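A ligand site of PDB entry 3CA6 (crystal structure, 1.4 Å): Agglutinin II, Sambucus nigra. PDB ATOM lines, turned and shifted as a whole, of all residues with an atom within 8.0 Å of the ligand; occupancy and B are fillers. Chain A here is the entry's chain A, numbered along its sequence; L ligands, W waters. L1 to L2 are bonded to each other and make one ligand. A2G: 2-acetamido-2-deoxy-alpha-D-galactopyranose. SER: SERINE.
Water W4 bridges an oxygen (OXT) of SER L2 (2.7 Å) and the side-chain amide oxygen of Gln 36 (3.4 Å). Water W2 lies within hydrogen-bond range of O6 of A2G L1 (2.8 Å), NH1 of Arg 107 (3.0 Å), OE1 of Gln 29 (3.0 Å) and NE of Arg 18 (3.4 Å). Water W1 lies within hydrogen-bond range of OD1 of Asn 38 (2.8 Å) and O7 of A2G L1 (3.4 Å).
Arg 18 touches the ligand. Gly 20 touches the ligand. NE1 of Trp 31 touches C3 of A2G L1, at 3.5 Å. NH1 of Arg 107 touches C6 of A2G L1, at 3.9 Å. Hydrophobic or aromatic side chains within 4 Å of the ligand: Trp 31. Of the 24 residues printed, 10 come within 4 Å of the ligand.
ND2 of Asn 38 sits at hydrogen-bond distance from OD2 of Asp 16 (3.3 Å). The backbone NH of Gln 29 lies within hydrogen-bond range of the backbone carbonyl oxygen of Asp 16 (2.9 Å). The side-chain amide nitrogen of Asn 38 sits at hydrogen-bond distance from the backbone carbonyl oxygen of Val 17 (2.9 Å). O of Trp 31 is in hydrogen-bond range of N of Cys 14, 2.8 Å away. O of Arg 107 lies within hydrogen-bond range of NH2 of Arg 18, 2.9 Å away. The backbone NH of Arg 18 lies within hydrogen-bond range of the backbone carbonyl oxygen of Pro 27 (3.1 Å). The backbone NH (N) of Arg 107 lies within hydrogen-bond range of the backbone carbonyl oxygen (O) of Leu 30 (2.8 Å). The side-chain sulfur of Cys 33 is disulfide-bonded to the side-chain sulfur of Cys 14, at 2.0 Å.
OD1 of Asp 16 lies within hydrogen-bond range of O3 of A2G L1, 2.6 Å away. O4 of A2G L1 sits at hydrogen-bond distance from N of Asn 19 (2.9 Å). OD1 of Asn 19 is in hydrogen-bond range of O6 of A2G L1, at 3.1 Å. The side-chain amide oxygen (OE1) of Gln 36 is in hydrogen-bond range of an oxygen (O3) of A2G L1 (2.9 Å). ND2 of Asn 38 is in hydrogen-bond range of O3 of A2G L1, at 2.9 Å. An oxygen (O6) of A2G L1 sits at hydrogen-bond distance from the side-chain amide nitrogen of Gln 29 (3.0 Å). The backbone carbonyl oxygen (O) of Val 17 sits at hydrogen-bond distance from an oxygen (O4) of A2G L1 (3.5 Å).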
ATOM      1  N   CYS A  14      22.429  -8.895  28.053  1.00  0.00           N
ATOM      2  CA  CYS A  14      21.765  -8.283  26.931  1.00  0.00           C
ATOM      3  C   CYS A  14      20.273  -8.622  26.913  1.00  0.00           C
ATOM      4  O   CYS A  14      19.908  -9.718  27.325  1.00  0.00           O
ATOM      5  CB  CYS A  14      22.463  -8.751  25.619  1.00  0.00           C
ATOM      6  SG  CYS A  14      23.902  -7.781  25.141  1.00  0.00           S
ATOM      7  N   VAL A  15      19.469  -7.715  26.352  1.00  0.00           N
ATOM      8  CA  VAL A  15      18.069  -7.901  26.081  1.00  0.00           C
ATOM      9  C   VAL A  15      17.898  -8.919  24.960  1.00  0.00           C
ATOM     10  O   VAL A  15      18.456  -8.779  23.866  1.00  0.00           O
ATOM     11  CB  VAL A  15      17.401  -6.570  25.696  1.00  0.00           C
ATOM     12  CG1 VAL A  15      15.874  -6.796  25.328  1.00  0.00           C
ATOM     13  CG2 VAL A  15      17.557  -5.545  26.808  1.00  0.00           C
ATOM     14  N   ASP A  16      17.184 -10.017  25.272  1.00  0.00           N
ATOM     15  CA  ASP A  16      17.174 -11.186  24.451  1.00  0.00           C
ATOM     16  C   ASP A  16      15.737 -11.743  24.370  1.00  0.00           C
ATOM     17  O   ASP A  16      15.065 -11.852  25.383  1.00  0.00           O
ATOM     18  CB  ASP A  16      18.100 -12.184  25.197  1.00  0.00           C
ATOM     19  CG  ASP A  16      18.216 -13.561  24.540  1.00  0.00           C
ATOM     20  OD1 ASP A  16      19.314 -13.939  24.013  1.00  0.00           O
ATOM     21  OD2 ASP A  16      17.228 -14.345  24.666  1.00  0.00           O
ATOM     22  N   VAL A  17      15.227 -12.027  23.163  1.00  0.00           N
ATOM     23  CA  VAL A  17      13.916 -12.670  23.013  1.00  0.00           C
ATOM     24  C   VAL A  17      14.056 -14.143  23.391  1.00  0.00           C
ATOM     25  O   VAL A  17      14.829 -14.900  22.785  1.00  0.00           O
ATOM     26  CB  VAL A  17      13.351 -12.495  21.631  1.00  0.00           C
ATOM     27  CG1 VAL A  17      11.889 -13.018  21.600  1.00  0.00           C
ATOM     28  CG2 VAL A  17      13.443 -11.015  21.215  1.00  0.00           C
ATOM     29  N   ARG A  18      13.304 -14.563  24.421  1.00  0.00           N
ATOM     30  CA  ARG A  18      13.516 -15.845  25.094  1.00  0.00           C
ATOM     31  C   ARG A  18      13.471 -17.030  24.127  1.00  0.00           C
ATOM     32  O   ARG A  18      12.493 -17.226  23.407  1.00  0.00           O
ATOM     33  CB  ARG A  18      12.471 -16.011  26.169  1.00  0.00           C
ATOM     34  CG  ARG A  18      12.773 -17.147  27.172  1.00  0.00           C
ATOM     35  CD  ARG A  18      11.959 -17.015  28.392  1.00  0.00           C
ATOM     36  NE  ARG A  18      12.251 -17.951  29.475  1.00  0.00           N
ATOM     37  CZ  ARG A  18      12.753 -17.631  30.663  1.00  0.00           C
ATOM     38  NH1 ARG A  18      12.780 -18.519  31.656  1.00  0.00           N
ATOM     39  NH2 ARG A  18      13.241 -16.409  30.890  1.00  0.00           N
ATOM     40  N   ASN A  19      14.523 -17.820  24.190  1.00  0.00           N
ATOM     41  CA  ASN A  19      14.716 -19.021  23.346  1.00  0.00           C
ATOM     42  C   ASN A  19      14.813 -18.738  21.890  1.00  0.00           C
ATOM     43  O   ASN A  19      14.824 -19.635  21.096  1.00  0.00           O
ATOM     44  CB  ASN A  19      13.594 -20.079  23.542  1.00  0.00           C
ATOM     45  CG  ASN A  19      13.269 -20.399  24.985  1.00  0.00           C
ATOM     46  OD1 ASN A  19      14.159 -20.685  25.779  1.00  0.00           O
ATOM     47  ND2 ASN A  19      11.988 -20.294  25.310  1.00  0.00           N
ATOM     48  N   GLY A  20      14.898 -17.460  21.504  1.00  0.00           N
ATOM     49  CA  GLY A  20      14.905 -17.184  20.066  1.00  0.00           C
ATOM     50  C   GLY A  20      13.600 -17.372  19.364  1.00  0.00           C
ATOM     51  O   GLY A  20      13.543 -17.314  18.121  1.00  0.00           O
ATOM     52  N   TYR A  21      12.536 -17.582  20.117  1.00  0.00           N
ATOM     53  CA  TYR A  21      11.210 -17.735  19.523  1.00  0.00           C
ATOM     54  C   TYR A  21      10.659 -16.407  19.068  1.00  0.00           C
ATOM     55  O   TYR A  21      10.846 -15.398  19.692  1.00  0.00           O
ATOM     56  CB  TYR A  21      10.219 -18.481  20.417  1.00  0.00           C
ATOM     57  CG  TYR A  21      10.627 -19.929  20.755  1.00  0.00           C
ATOM     58  CD1 TYR A  21       9.914 -20.646  21.701  1.00  0.00           C
ATOM     59  CD2 TYR A  21      11.713 -20.590  20.135  1.00  0.00           C
ATOM     60  CE1 TYR A  21      10.263 -21.964  22.034  1.00  0.00           C
ATOM     61  CE2 TYR A  21      12.038 -21.936  20.462  1.00  0.00           C
ATOM     62  CZ  TYR A  21      11.306 -22.584  21.436  1.00  0.00           C
ATOM     63  OH  TYR A  21      11.567 -23.907  21.762  1.00  0.00           O
ATOM     64  N   THR A  26       6.200 -13.747  23.135  1.00  0.00           N
ATOM     65  CA  THR A  26       7.469 -14.290  23.720  1.00  0.00           C
ATOM     66  C   THR A  26       8.120 -13.223  24.577  1.00  0.00           C
ATOM     67  O   THR A  26       8.347 -12.141  24.086  1.00  0.00           O
ATOM     68  CB  THR A  26       8.427 -14.780  22.657  1.00  0.00           C
ATOM     69  OG1 THR A  26       7.766 -15.790  21.844  1.00  0.00           O
ATOM     70  CG2 THR A  26       9.671 -15.314  23.293  1.00  0.00           C
ATOM     71  N   PRO A  27       8.292 -13.430  25.865  1.00  0.00           N
ATOM     72  CA  PRO A  27       8.946 -12.417  26.714  1.00  0.00           C
ATOM     73  C   PRO A  27      10.381 -12.133  26.358  1.00  0.00           C
ATOM     74  O   PRO A  27      11.051 -12.918  25.667  1.00  0.00           O
ATOM     75  CB  PRO A  27       8.871 -13.013  28.120  1.00  0.00           C
ATOM     76  CG  PRO A  27       8.253 -14.437  27.958  1.00  0.00           C
ATOM     77  CD  PRO A  27       7.789 -14.601  26.609  1.00  0.00           C
ATOM     78  N   GLN A  29      14.122 -11.208  28.022  1.00  0.00           N
ATOM     79  CA  GLN A  29      14.889 -11.617  29.168  1.00  0.00           C
ATOM     80  C   GLN A  29      16.322 -11.045  29.100  1.00  0.00           C
ATOM     81  O   GLN A  29      16.738 -10.566  28.064  1.00  0.00           O
ATOM     82  CB  GLN A  29      14.948 -13.175  29.208  1.00  0.00           C
ATOM     83  CG  GLN A  29      15.771 -13.774  28.108  1.00  0.00           C
ATOM     84  CD  GLN A  29      15.902 -15.247  28.164  1.00  0.00           C
ATOM     85  OE1 GLN A  29      15.421 -15.901  29.097  1.00  0.00           O
ATOM     86  NE2 GLN A  29      16.544 -15.820  27.130  1.00  0.00           N
ATOM     87  N   LEU A  30      17.074 -11.231  30.165  1.00  0.00           N
ATOM     88  CA  LEU A  30      18.518 -11.082  30.143  1.00  0.00           C
ATOM     89  C   LEU A  30      19.171 -12.395  29.728  1.00  0.00           C
ATOM     90  O   LEU A  30      18.808 -13.467  30.179  1.00  0.00           O
ATOM     91  CB  LEU A  30      19.038 -10.676  31.521  1.00  0.00           C
ATOM     92  CG  LEU A  30      18.610  -9.371  32.188  1.00  0.00           C
ATOM     93  CD1 LEU A  30      19.357  -9.357  33.556  1.00  0.00           C
ATOM     94  CD2 LEU A  30      18.969  -8.271  31.265  1.00  0.00           C
ATOM     95  N   TRP A  31      20.213 -12.266  28.922  1.00  0.00           N
ATOM     96  CA  TRP A  31      21.043 -13.417  28.520  1.00  0.00           C
ATOM     97  C   TRP A  31      22.435 -12.878  28.157  1.00  0.00           C
ATOM     98  O   TRP A  31      22.554 -11.716  27.720  1.00  0.00           O
ATOM     99  CB  TRP A  31      20.379 -14.105  27.310  1.00  0.00           C
ATOM    100  CG  TRP A  31      20.955 -15.410  26.945  1.00  0.00           C
ATOM    101  CD1 TRP A  31      21.696 -15.693  25.845  1.00  0.00           C
ATOM    102  CD2 TRP A  31      20.773 -16.663  27.618  1.00  0.00           C
ATOM    103  NE1 TRP A  31      22.048 -17.014  25.836  1.00  0.00           N
ATOM    104  CE2 TRP A  31      21.470 -17.632  26.896  1.00  0.00           C
ATOM    105  CE3 TRP A  31      20.143 -17.047  28.793  1.00  0.00           C
ATOM    106  CZ2 TRP A  31      21.576 -18.948  27.315  1.00  0.00           C
ATOM    107  CZ3 TRP A  31      20.226 -18.367  29.204  1.00  0.00           C
ATOM    108  CH2 TRP A  31      20.953 -19.289  28.473  1.00  0.00           C
ATOM    109  N   PRO A  32      23.471 -13.701  28.302  1.00  0.00           N
ATOM    110  CA  PRO A  32      24.791 -13.238  27.929  1.00  0.00           C
ATOM    111  C   PRO A  32      24.834 -12.753  26.502  1.00  0.00           C
ATOM    112  O   PRO A  32      24.203 -13.301  25.587  1.00  0.00           O
ATOM    113  CB  PRO A  32      25.666 -14.493  28.122  1.00  0.00           C
ATOM    114  CG  PRO A  32      25.028 -15.221  29.209  1.00  0.00           C
ATOM    115  CD  PRO A  32      23.540 -15.016  28.951  1.00  0.00           C
ATOM    116  N   CYS A  33      25.487 -11.615  26.280  1.00  0.00           N
ATOM    117  CA  CYS A  33      25.466 -10.975  25.006  1.00  0.00           C
ATOM    118  C   CYS A  33      26.147 -11.812  23.916  1.00  0.00           C
ATOM    119  O   CYS A  33      27.212 -12.423  24.110  1.00  0.00           O
ATOM    120  CB  CYS A  33      26.165  -9.619  25.082  1.00  0.00           C
ATOM    121  SG  CYS A  33      25.468  -8.409  26.155  1.00  0.00           S
ATOM    122  N   GLY A  34      25.532 -11.738  22.764  1.00  0.00           N
ATOM    123  CA  GLY A  34      25.991 -12.425  21.557  1.00  0.00           C
ATOM    124  C   GLY A  34      25.410 -11.777  20.327  1.00  0.00           C
ATOM    125  O   GLY A  34      24.752 -10.740  20.370  1.00  0.00           O
ATOM    126  N   THR A  35      25.668 -12.424  19.189  1.00  0.00           N
ATOM    127  CA  THR A  35      25.262 -11.949  17.906  1.00  0.00           C
ATOM    128  C   THR A  35      23.968 -12.514  17.351  1.00  0.00           C
ATOM    129  O   THR A  35      23.560 -12.184  16.263  1.00  0.00           O
ATOM    130  CB  THR A  35      26.434 -12.274  16.859  1.00  0.00           C
ATOM    131  OG1 THR A  35      26.673 -13.708  16.856  1.00  0.00           O
ATOM    132  CG2 THR A  35      27.730 -11.619  17.276  1.00  0.00           C
ATOM    133  N   GLN A  36      23.357 -13.414  18.082  1.00  0.00           N
ATOM    134  CA  GLN A  36      22.150 -14.039  17.628  1.00  0.00           C
ATOM    135  C   GLN A  36      21.062 -13.002  17.327  1.00  0.00           C
ATOM    136  O   GLN A  36      20.941 -11.961  17.983  1.00  0.00           O
ATOM    137  CB  GLN A  36      21.689 -15.136  18.618  1.00  0.00           C
ATOM    138  CG  GLN A  36      21.487 -14.623  20.074  1.00  0.00           C
ATOM    139  CD  GLN A  36      22.653 -14.953  21.009  1.00  0.00           C
ATOM    140  OE1 GLN A  36      22.464 -15.461  22.153  1.00  0.00           O
ATOM    141  NE2 GLN A  36      23.833 -14.679  20.560  1.00  0.00           N
ATOM    142  N   ARG A  37      20.210 -13.298  16.380  1.00  0.00           N
ATOM    143  CA  ARG A  37      19.274 -12.339  15.869  1.00  0.00           C
ATOM    144  C   ARG A  37      18.264 -11.835  16.882  1.00  0.00           C
ATOM    145  O   ARG A  37      17.755 -10.760  16.776  1.00  0.00           O
ATOM    146  CB  ARG A  37      18.577 -12.877  14.588  1.00  0.00           C
ATOM    147  CG  ARG A  37      19.536 -13.271  13.498  1.00  0.00           C
ATOM    148  CD  ARG A  37      20.589 -12.214  13.161  1.00  0.00           C
ATOM    149  NE  ARG A  37      19.959 -10.942  12.768  1.00  0.00           N
ATOM    150  CZ  ARG A  37      20.675  -9.837  12.584  1.00  0.00           C
ATOM    151  NH1 ARG A  37      20.084  -8.697  12.247  1.00  0.00           N
ATOM    152  NH2 ARG A  37      22.001  -9.893  12.688  1.00  0.00           N
ATOM    153  N   ASN A  38      17.948 -12.707  17.844  1.00  0.00           N
ATOM    154  CA  ASN A  38      17.023 -12.352  18.971  1.00  0.00           C
ATOM    155  C   ASN A  38      17.666 -11.450  20.038  1.00  0.00           C
ATOM    156  O   ASN A  38      17.001 -11.112  21.018  1.00  0.00           O
ATOM    157  CB  ASN A  38      16.451 -13.651  19.574  1.00  0.00           C
ATOM    158  CG  ASN A  38      17.488 -14.574  20.075  1.00  0.00           C
ATOM    159  OD1 ASN A  38      18.411 -14.983  19.347  1.00  0.00           O
ATOM    160  ND2 ASN A  38      17.403 -14.928  21.387  1.00  0.00           N
ATOM    161  N   GLN A  39      18.915 -10.985  19.784  1.00  0.00           N
ATOM    162  CA  GLN A  39      19.552  -9.917  20.561  1.00  0.00           C
ATOM    163  C   GLN A  39      19.852  -8.689  19.673  1.00  0.00           C
ATOM    164  O   GLN A  39      20.409  -7.752  20.175  1.00  0.00           O
ATOM    165  CB  GLN A  39      20.833 -10.423  21.200  1.00  0.00           C
ATOM    166  CG  GLN A  39      20.621 -11.268  22.411  1.00  0.00           C
ATOM    167  CD  GLN A  39      21.845 -11.472  23.231  1.00  0.00           C
ATOM    168  OE1 GLN A  39      22.834 -10.720  23.078  1.00  0.00           O
ATOM    169  NE2 GLN A  39      21.851 -12.504  24.075  1.00  0.00           N
ATOM    170  N   MET A  52      13.730  -9.661  14.992  1.00  0.00           N
ATOM    171  CA  MET A  52      13.113 -10.728  14.205  1.00  0.00           C
ATOM    172  C   MET A  52      11.842 -10.295  13.488  1.00  0.00           C
ATOM    173  O   MET A  52      10.918 -11.080  13.213  1.00  0.00           O
ATOM    174  CB  MET A  52      12.852 -11.944  15.103  1.00  0.00           C
ATOM    175  CG  MET A  52      14.171 -12.525  15.617  1.00  0.00           C
ATOM    176  SD  MET A  52      13.934 -13.960  16.646  1.00  0.00           S
ATOM    177  CE  MET A  52      12.953 -13.270  17.915  1.00  0.00           C
ATOM    178  N   SER A 106      20.877 -14.420  34.461  1.00  0.00           N
ATOM    179  CA  SER A 106      20.398 -14.781  33.137  1.00  0.00           C
ATOM    180  C   SER A 106      19.004 -15.399  33.313  1.00  0.00           C
ATOM    181  O   SER A 106      18.699 -15.997  34.362  1.00  0.00           O
ATOM    182  CB  SER A 106      21.322 -15.738  32.430  1.00  0.00           C
ATOM    183  OG  SER A 106      21.282 -17.013  33.061  1.00  0.00           O
ATOM    184  N   ARG A 107      18.177 -15.252  32.277  1.00  0.00           N
ATOM    185  CA  ARG A 107      16.812 -15.725  32.211  1.00  0.00           C
ATOM    186  C   ARG A 107      15.835 -14.900  33.062  1.00  0.00           C
ATOM    187  O   ARG A 107      14.624 -15.168  33.063  1.00  0.00           O
ATOM    188  CB  ARG A 107      16.597 -17.194  32.419  1.00  0.00           C
ATOM    189  CG  ARG A 107      17.498 -18.130  31.621  1.00  0.00           C
ATOM    190  CD  ARG A 107      17.228 -19.622  32.048  1.00  0.00           C
ATOM    191  NE  ARG A 107      18.299 -20.547  31.629  1.00  0.00           N
ATOM    192  CZ  ARG A 107      18.314 -21.239  30.517  1.00  0.00           C
ATOM    193  NH1 ARG A 107      17.349 -21.173  29.660  1.00  0.00           N
ATOM    194  NH2 ARG A 107      19.321 -22.048  30.260  1.00  0.00           N
HETATM  195  O5  A2G L   1      18.060 -19.715  24.110  1.00  0.00           O
HETATM  196  C1  A2G L   1      18.763 -19.785  22.853  1.00  0.00           C
HETATM  197  C2  A2G L   1      18.977 -18.375  22.302  1.00  0.00           C
HETATM  198  N2  A2G L   1      19.797 -18.418  21.086  1.00  0.00           N
HETATM  199  C3  A2G L   1      19.549 -17.431  23.355  1.00  0.00           C
HETATM  200  O3  A2G L   1      19.709 -16.143  22.748  1.00  0.00           O
HETATM  201  C4  A2G L   1      18.581 -17.400  24.553  1.00  0.00           C
HETATM  202  O4  A2G L   1      17.282 -16.946  24.192  1.00  0.00           O
HETATM  203  C5  A2G L   1      18.597 -18.843  25.116  1.00  0.00           C
HETATM  204  C6  A2G L   1      17.836 -18.987  26.478  1.00  0.00           C
HETATM  205  O6  A2G L   1      16.448 -18.700  26.313  1.00  0.00           O
HETATM  206  C7  A2G L   1      19.264 -18.531  19.851  1.00  0.00           C
HETATM  207  O7  A2G L   1      18.078 -18.633  19.657  1.00  0.00           O
HETATM  208  C8  A2G L   1      20.282 -18.672  18.730  1.00  0.00           C
HETATM  209  N   SER L   2      22.389 -21.779  24.120  1.00  0.00           N
HETATM  210  CA  SER L   2      21.353 -22.327  23.197  1.00  0.00           C
HETATM  211  C   SER L   2      21.721 -22.073  21.735  1.00  0.00           C
HETATM  212  O   SER L   2      21.055 -22.487  20.780  1.00  0.00           O
HETATM  213  CB  SER L   2      19.996 -21.729  23.537  1.00  0.00           C
HETATM  214  OG  SER L   2      19.970 -20.372  23.106  1.00  0.00           O
HETATM  215  OXT SER L   2      22.707 -21.408  21.472  1.00  0.00           O
HETATM  216  O   HOH W   1      18.053 -16.492  16.963  1.00  0.00           O
HETATM  217  O   HOH W   2      15.497 -18.917  28.954  1.00  0.00           O
HETATM  218  O   HOH W   3      20.901 -22.650  26.756  1.00  0.00           O
HETATM  219  O   HOH W   4      22.619 -18.696  21.254  1.00  0.00           O
